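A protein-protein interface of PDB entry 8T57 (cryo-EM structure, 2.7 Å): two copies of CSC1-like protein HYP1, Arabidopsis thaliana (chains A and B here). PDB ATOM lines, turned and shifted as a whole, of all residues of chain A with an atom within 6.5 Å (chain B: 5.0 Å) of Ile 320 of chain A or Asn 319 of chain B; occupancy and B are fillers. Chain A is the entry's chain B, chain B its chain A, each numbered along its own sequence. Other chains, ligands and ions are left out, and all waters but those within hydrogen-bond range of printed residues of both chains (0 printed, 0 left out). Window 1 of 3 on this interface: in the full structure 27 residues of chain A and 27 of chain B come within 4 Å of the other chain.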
ATOM      1  N   HIS A 216      -4.997 -12.833 -11.917  1.00  0.00           N
ATOM      2  CA  HIS A 216      -5.556 -12.378 -13.180  1.00  0.00           C
ATOM      3  C   HIS A 216      -5.493 -13.509 -14.180  1.00  0.00           C
ATOM      4  O   HIS A 216      -5.047 -13.338 -15.318  1.00  0.00           O
ATOM      5  CB  HIS A 216      -4.751 -11.208 -13.700  1.00  0.00           C
ATOM      6  CG  HIS A 216      -4.788 -10.093 -12.832  1.00  0.00           C
ATOM      7  ND1 HIS A 216      -5.781  -9.182 -12.857  1.00  0.00           N
ATOM      8  CD2 HIS A 216      -3.981  -9.736 -11.860  1.00  0.00           C
ATOM      9  CE1 HIS A 216      -5.558  -8.295 -11.941  1.00  0.00           C
ATOM     10  NE2 HIS A 216      -4.476  -8.617 -11.330  1.00  0.00           N
ATOM     11  N   ALA A 315      -6.923  -2.657 -17.469  1.00  0.00           N
ATOM     12  CA  ALA A 315      -7.488  -1.615 -16.638  1.00  0.00           C
ATOM     13  C   ALA A 315      -7.706  -2.103 -15.236  1.00  0.00           C
ATOM     14  O   ALA A 315      -7.554  -1.346 -14.283  1.00  0.00           O
ATOM     15  CB  ALA A 315      -8.803  -1.137 -17.210  1.00  0.00           C
ATOM     16  N   ILE A 316      -8.086  -3.350 -15.084  1.00  0.00           N
ATOM     17  CA  ILE A 316      -8.297  -3.875 -13.762  1.00  0.00           C
ATOM     18  C   ILE A 316      -6.959  -3.958 -13.049  1.00  0.00           C
ATOM     19  O   ILE A 316      -6.823  -3.505 -11.911  1.00  0.00           O
ATOM     20  CB  ILE A 316      -9.014  -5.210 -13.835  1.00  0.00           C
ATOM     21  CG1 ILE A 316     -10.412  -4.960 -14.350  1.00  0.00           C
ATOM     22  CG2 ILE A 316      -9.042  -5.846 -12.480  1.00  0.00           C
ATOM     23  CD1 ILE A 316     -11.124  -6.163 -14.784  1.00  0.00           C
ATOM     24  N   ALA A 317      -5.937  -4.472 -13.723  1.00  0.00           N
ATOM     25  CA  ALA A 317      -4.625  -4.563 -13.095  1.00  0.00           C
ATOM     26  C   ALA A 317      -4.099  -3.204 -12.664  1.00  0.00           C
ATOM     27  O   ALA A 317      -3.473  -3.114 -11.617  1.00  0.00           O
ATOM     28  CB  ALA A 317      -3.640  -5.206 -14.020  1.00  0.00           C
ATOM     29  N   THR A 318      -4.372  -2.145 -13.418  1.00  0.00           N
ATOM     30  CA  THR A 318      -3.892  -0.828 -13.034  1.00  0.00           C
ATOM     31  C   THR A 318      -4.826  -0.025 -12.154  1.00  0.00           C
ATOM     32  O   THR A 318      -4.376   0.904 -11.486  1.00  0.00           O
ATOM     33  CB  THR A 318      -3.568   0.042 -14.249  1.00  0.00           C
ATOM     34  OG1 THR A 318      -4.724   0.207 -15.056  1.00  0.00           O
ATOM     35  CG2 THR A 318      -2.516  -0.576 -15.035  1.00  0.00           C
ATOM     36  N   ASN A 319      -6.114  -0.346 -12.113  1.00  0.00           N
ATOM     37  CA  ASN A 319      -7.020   0.471 -11.327  1.00  0.00           C
ATOM     38  C   ASN A 319      -7.301  -0.047  -9.927  1.00  0.00           C
ATOM     39  O   ASN A 319      -7.648   0.732  -9.040  1.00  0.00           O
ATOM     40  CB  ASN A 319      -8.307   0.660 -12.072  1.00  0.00           C
ATOM     41  CG  ASN A 319      -8.125   1.476 -13.309  1.00  0.00           C
ATOM     42  OD1 ASN A 319      -7.333   2.417 -13.365  1.00  0.00           O
ATOM     43  ND2 ASN A 319      -8.847   1.131 -14.318  1.00  0.00           N
ATOM     44  N   ILE A 320      -7.144  -1.338  -9.699  1.00  0.00           N
ATOM     45  CA  ILE A 320      -7.438  -1.889  -8.392  1.00  0.00           C
ATOM     46  C   ILE A 320      -6.157  -2.296  -7.681  1.00  0.00           C
ATOM     47  O   ILE A 320      -5.319  -2.995  -8.240  1.00  0.00           O
ATOM     48  CB  ILE A 320      -8.444  -3.054  -8.500  1.00  0.00           C
ATOM     49  CG1 ILE A 320      -9.745  -2.490  -9.089  1.00  0.00           C
ATOM     50  CG2 ILE A 320      -8.680  -3.718  -7.141  1.00  0.00           C
ATOM     51  CD1 ILE A 320     -10.806  -3.476  -9.429  1.00  0.00           C
ATOM     52  N   GLN A 321      -5.998  -1.859  -6.423  1.00  0.00           N
ATOM     53  CA  GLN A 321      -4.801  -2.195  -5.646  1.00  0.00           C
ATOM     54  C   GLN A 321      -4.588  -3.674  -5.733  1.00  0.00           C
ATOM     55  O   GLN A 321      -5.550  -4.435  -5.619  1.00  0.00           O
ATOM     56  CB  GLN A 321      -4.950  -1.818  -4.188  1.00  0.00           C
ATOM     57  CG  GLN A 321      -3.731  -2.108  -3.335  1.00  0.00           C
ATOM     58  CD  GLN A 321      -3.995  -1.773  -1.947  1.00  0.00           C
ATOM     59  OE1 GLN A 321      -4.603  -0.742  -1.680  1.00  0.00           O
ATOM     60  NE2 GLN A 321      -3.592  -2.626  -1.034  1.00  0.00           N
ATOM     61  N   GLN A 322      -3.347  -4.075  -5.975  1.00  0.00           N
ATOM     62  CA  GLN A 322      -3.050  -5.471  -6.175  1.00  0.00           C
ATOM     63  C   GLN A 322      -2.623  -6.244  -4.954  1.00  0.00           C
ATOM     64  O   GLN A 322      -3.275  -7.214  -4.578  1.00  0.00           O
ATOM     65  CB  GLN A 322      -1.973  -5.565  -7.238  1.00  0.00           C
ATOM     66  CG  GLN A 322      -2.423  -5.114  -8.584  1.00  0.00           C
ATOM     67  CD  GLN A 322      -3.410  -6.009  -9.175  1.00  0.00           C
ATOM     68  OE1 GLN A 322      -3.124  -7.177  -9.385  1.00  0.00           O
ATOM     69  NE2 GLN A 322      -4.586  -5.515  -9.424  1.00  0.00           N
ATOM     70  N   GLY A 323      -1.547  -5.867  -4.316  1.00  0.00           N
ATOM     71  CA  GLY A 323      -1.112  -6.686  -3.201  1.00  0.00           C
ATOM     72  C   GLY A 323      -1.682  -6.200  -1.896  1.00  0.00           C
ATOM     73  O   GLY A 323      -2.265  -5.116  -1.847  1.00  0.00           O
ATOM     74  N   THR A 331       1.106  -0.886 -10.041  1.00  0.00           N
ATOM     75  CA  THR A 331       0.836  -1.027 -11.453  1.00  0.00           C
ATOM     76  C   THR A 331       0.506   0.288 -12.135  1.00  0.00           C
ATOM     77  O   THR A 331      -0.257   1.105 -11.622  1.00  0.00           O
ATOM     78  CB  THR A 331      -0.304  -2.005 -11.607  1.00  0.00           C
ATOM     79  OG1 THR A 331      -1.380  -1.531 -10.835  1.00  0.00           O
ATOM     80  CG2 THR A 331       0.081  -3.374 -11.135  1.00  0.00           C
ATOM     81  N   HIS B 312     -14.754  -9.733  -5.777  1.00  0.00           N
ATOM     82  CA  HIS B 312     -13.890  -9.096  -6.746  1.00  0.00           C
ATOM     83  C   HIS B 312     -14.756  -8.479  -7.840  1.00  0.00           C
ATOM     84  O   HIS B 312     -14.538  -7.340  -8.249  1.00  0.00           O
ATOM     85  CB  HIS B 312     -12.876 -10.073  -7.310  1.00  0.00           C
ATOM     86  CG  HIS B 312     -11.871  -9.427  -8.157  1.00  0.00           C
ATOM     87  ND1 HIS B 312     -10.977  -8.507  -7.663  1.00  0.00           N
ATOM     88  CD2 HIS B 312     -11.578  -9.570  -9.447  1.00  0.00           C
ATOM     89  CE1 HIS B 312     -10.197  -8.105  -8.623  1.00  0.00           C
ATOM     90  NE2 HIS B 312     -10.530  -8.738  -9.713  1.00  0.00           N
ATOM     91  N   ALA B 314     -17.777  -7.281  -7.652  1.00  0.00           N
ATOM     92  CA  ALA B 314     -18.364  -6.049  -7.184  1.00  0.00           C
ATOM     93  C   ALA B 314     -17.326  -4.961  -7.122  1.00  0.00           C
ATOM     94  O   ALA B 314     -17.591  -3.835  -7.526  1.00  0.00           O
ATOM     95  CB  ALA B 314     -18.992  -6.254  -5.836  1.00  0.00           C
ATOM     96  N   ALA B 315     -16.109  -5.297  -6.723  1.00  0.00           N
ATOM     97  CA  ALA B 315     -15.056  -4.309  -6.637  1.00  0.00           C
ATOM     98  C   ALA B 315     -14.802  -3.674  -7.974  1.00  0.00           C
ATOM     99  O   ALA B 315     -14.488  -2.491  -8.050  1.00  0.00           O
ATOM    100  CB  ALA B 315     -13.777  -4.939  -6.134  1.00  0.00           C
ATOM    101  N   ILE B 316     -14.906  -4.440  -9.034  1.00  0.00           N
ATOM    102  CA  ILE B 316     -14.688  -3.882 -10.342  1.00  0.00           C
ATOM    103  C   ILE B 316     -15.811  -2.911 -10.654  1.00  0.00           C
ATOM    104  O   ILE B 316     -15.567  -1.780 -11.076  1.00  0.00           O
ATOM    105  CB  ILE B 316     -14.558  -4.990 -11.369  1.00  0.00           C
ATOM    106  CG1 ILE B 316     -13.281  -5.745 -11.083  1.00  0.00           C
ATOM    107  CG2 ILE B 316     -14.541  -4.403 -12.748  1.00  0.00           C
ATOM    108  CD1 ILE B 316     -13.168  -7.030 -11.773  1.00  0.00           C
ATOM    109  N   ALA B 317     -17.052  -3.304 -10.389  1.00  0.00           N
ATOM    110  CA  ALA B 317     -18.170  -2.408 -10.654  1.00  0.00           C
ATOM    111  C   ALA B 317     -18.057  -1.104  -9.882  1.00  0.00           C
ATOM    112  O   ALA B 317     -18.410  -0.064 -10.419  1.00  0.00           O
ATOM    113  CB  ALA B 317     -19.469  -3.071 -10.316  1.00  0.00           C
ATOM    114  N   THR B 318     -17.534  -1.128  -8.661  1.00  0.00           N
ATOM    115  CA  THR B 318     -17.402   0.101  -7.896  1.00  0.00           C
ATOM    116  C   THR B 318     -16.096   0.846  -8.079  1.00  0.00           C
ATOM    117  O   THR B 318     -16.036   2.038  -7.789  1.00  0.00           O
ATOM    118  CB  THR B 318     -17.574  -0.135  -6.394  1.00  0.00           C
ATOM    119  OG1 THR B 318     -16.599  -1.056  -5.930  1.00  0.00           O
ATOM    120  CG2 THR B 318     -18.899  -0.658  -6.124  1.00  0.00           C
ATOM    121  N   ASN B 319     -15.042   0.195  -8.557  1.00  0.00           N
ATOM    122  CA  ASN B 319     -13.771   0.891  -8.661  1.00  0.00           C
ATOM    123  C   ASN B 319     -13.473   1.483 -10.027  1.00  0.00           C
ATOM    124  O   ASN B 319     -12.708   2.440 -10.131  1.00  0.00           O
ATOM    125  CB  ASN B 319     -12.658  -0.023  -8.242  1.00  0.00           C
ATOM    126  CG  ASN B 319     -12.725  -0.360  -6.790  1.00  0.00           C
ATOM    127  OD1 ASN B 319     -13.097   0.453  -5.942  1.00  0.00           O
ATOM    128  ND2 ASN B 319     -12.375  -1.559  -6.478  1.00  0.00           N
ATOM    129  N   ILE B 320     -14.068   0.949 -11.079  1.00  0.00           N
ATOM    130  CA  ILE B 320     -13.787   1.449 -12.409  1.00  0.00           C
ATOM    131  C   ILE B 320     -14.983   2.209 -12.960  1.00  0.00           C
ATOM    132  O   ILE B 320     -16.106   1.718 -12.938  1.00  0.00           O
ATOM    133  CB  ILE B 320     -13.335   0.307 -13.342  1.00  0.00           C
ATOM    134  CG1 ILE B 320     -12.039  -0.281 -12.763  1.00  0.00           C
ATOM    135  CG2 ILE B 320     -13.140   0.800 -14.778  1.00  0.00           C
ATOM    136  CD1 ILE B 320     -11.510  -1.505 -13.421  1.00  0.00           C
ATOM    137  N   GLN B 321     -14.744   3.425 -13.473  1.00  0.00           N
ATOM    138  CA  GLN B 321     -15.826   4.240 -14.033  1.00  0.00           C
ATOM    139  C   GLN B 321     -16.599   3.394 -14.996  1.00  0.00           C
ATOM    140  O   GLN B 321     -15.995   2.663 -15.782  1.00  0.00           O
ATOM    141  CB  GLN B 321     -15.296   5.448 -14.776  1.00  0.00           C
ATOM    142  CG  GLN B 321     -16.367   6.354 -15.351  1.00  0.00           C
ATOM    143  CD  GLN B 321     -15.760   7.442 -16.097  1.00  0.00           C
ATOM    144  OE1 GLN B 321     -14.770   8.004 -15.645  1.00  0.00           O
ATOM    145  NE2 GLN B 321     -16.296   7.748 -17.256  1.00  0.00           N
ATOM    146  N   THR B 660      -6.856  -6.820  -4.549  1.00  0.00           N
ATOM    147  CA  THR B 660      -7.095  -7.998  -5.353  1.00  0.00           C
ATOM    148  C   THR B 660      -6.543  -9.235  -4.712  1.00  0.00           C
ATOM    149  O   THR B 660      -7.243 -10.228  -4.600  1.00  0.00           O
ATOM    150  CB  THR B 660      -6.466  -7.848  -6.745  1.00  0.00           C
ATOM    151  OG1 THR B 660      -7.080  -6.760  -7.427  1.00  0.00           O
ATOM    152  CG2 THR B 660      -6.637  -9.101  -7.547  1.00  0.00           C
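Ala 315 of chain A touches none of the printed residues of chain B.
Of the printed residues of chain B, Asn 319 of chain A touches Ile 320 (3.8 Å).
Of chain B, only Ile 316 (3.7 Å), Asn 319 (3.8 Å) and Thr 660 (3.4 Å) come within 4 Å of Ile 320 of chain A.
Of the printed residues of chain B, Gln 322 of chain A touches Thr 660.
Ala 317 of chain B touches none of the printed residues of chain A.
Of chain A, only Ile 320 comes within 4 Å of Asn 319 of chain B.
The nearest residue of chain A that does not touch Asn 319 of chain B is Asn 319 of chain A (5.1 Å).
Ile 316 of chain A touches its own counterpart, Ile 316 of chain B.
Ile 316 of chain A touches Ile 320 of chain B, and with the chains exchanged Ile 320 of chain A touches Ile 316 of chain B.
Asn 319 of chain A touches Ile 320 of chain B, and with the chains exchanged Ile 320 of chain A touches Asn 319 of chain B.
Positions printed for both chains: 315, 316, 317, 318, 319, 320 and 321.
The backbone NH (N) of Thr 660 of chain B sits at hydrogen-bond distance from the backbone carbonyl oxygen (O) of Gln 321 of chain A (2.9 Å).
The side-chain amide nitrogen of Gln 322 of chain A lies within hydrogen-bond range of the side-chain hydroxyl of Thr 660 of chain B, 3.4 Å away.
Of the 10 printed residues of chain B, 4 touch a printed residue of chain A.
Hydrophobic or aromatic side chains of chain B that line the printed part of chain A: Ile 316 and Ile 320.
Of the 11 printed residues of chain A, 5 touch a printed residue of chain B.
Among the printed residues, 8 pairs touch across the chains.
The backbone carbonyl oxygen of Ala 315 of chain A is in hydrogen-bond range of the side-chain amide nitrogen of Asn 319 of chain A (2.8 Å).
A ring nitrogen (NE2) of His 216 of chain A is in hydrogen-bond range of the side-chain amide oxygen of Gln 322 of chain A, 2.8 Å away.
The backbone carbonyl oxygen (O) of Ile 320 of chain A is in hydrogen-bond range of the side-chain amide nitrogen (NE2) of Gln 322 of chain A.
O of Gly 323 of chain A is in hydrogen-bond range of NE2 of Gln 321 of chain A, 2.9 Å away.
NE2 of Gln 322 of chain A sits at hydrogen-bond distance from O of Ala 317 of chain A, 3.4 Å away.
ND2 of Asn 319 of chain B sits at hydrogen-bond distance from O of Ala 315 of chain B, at 2.8 Å.
Among the printed residues, merely in contact across the chains: Ile 320 of chain A with Thr 660 of chain B (3.4 Å), Ile 316 of chain A with Ile 316 of chain B (3.7 Å), Ile 316 of chain A with Ile 320 of chain B (3.7 Å), Ile 320 of chain A with Ile 316 of chain B (3.7 Å), Asn 319 of chain A with Ile 320 of chain B (3.8 Å) and Ile 320 of chain A with Asn 319 of chain B (3.8 Å).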
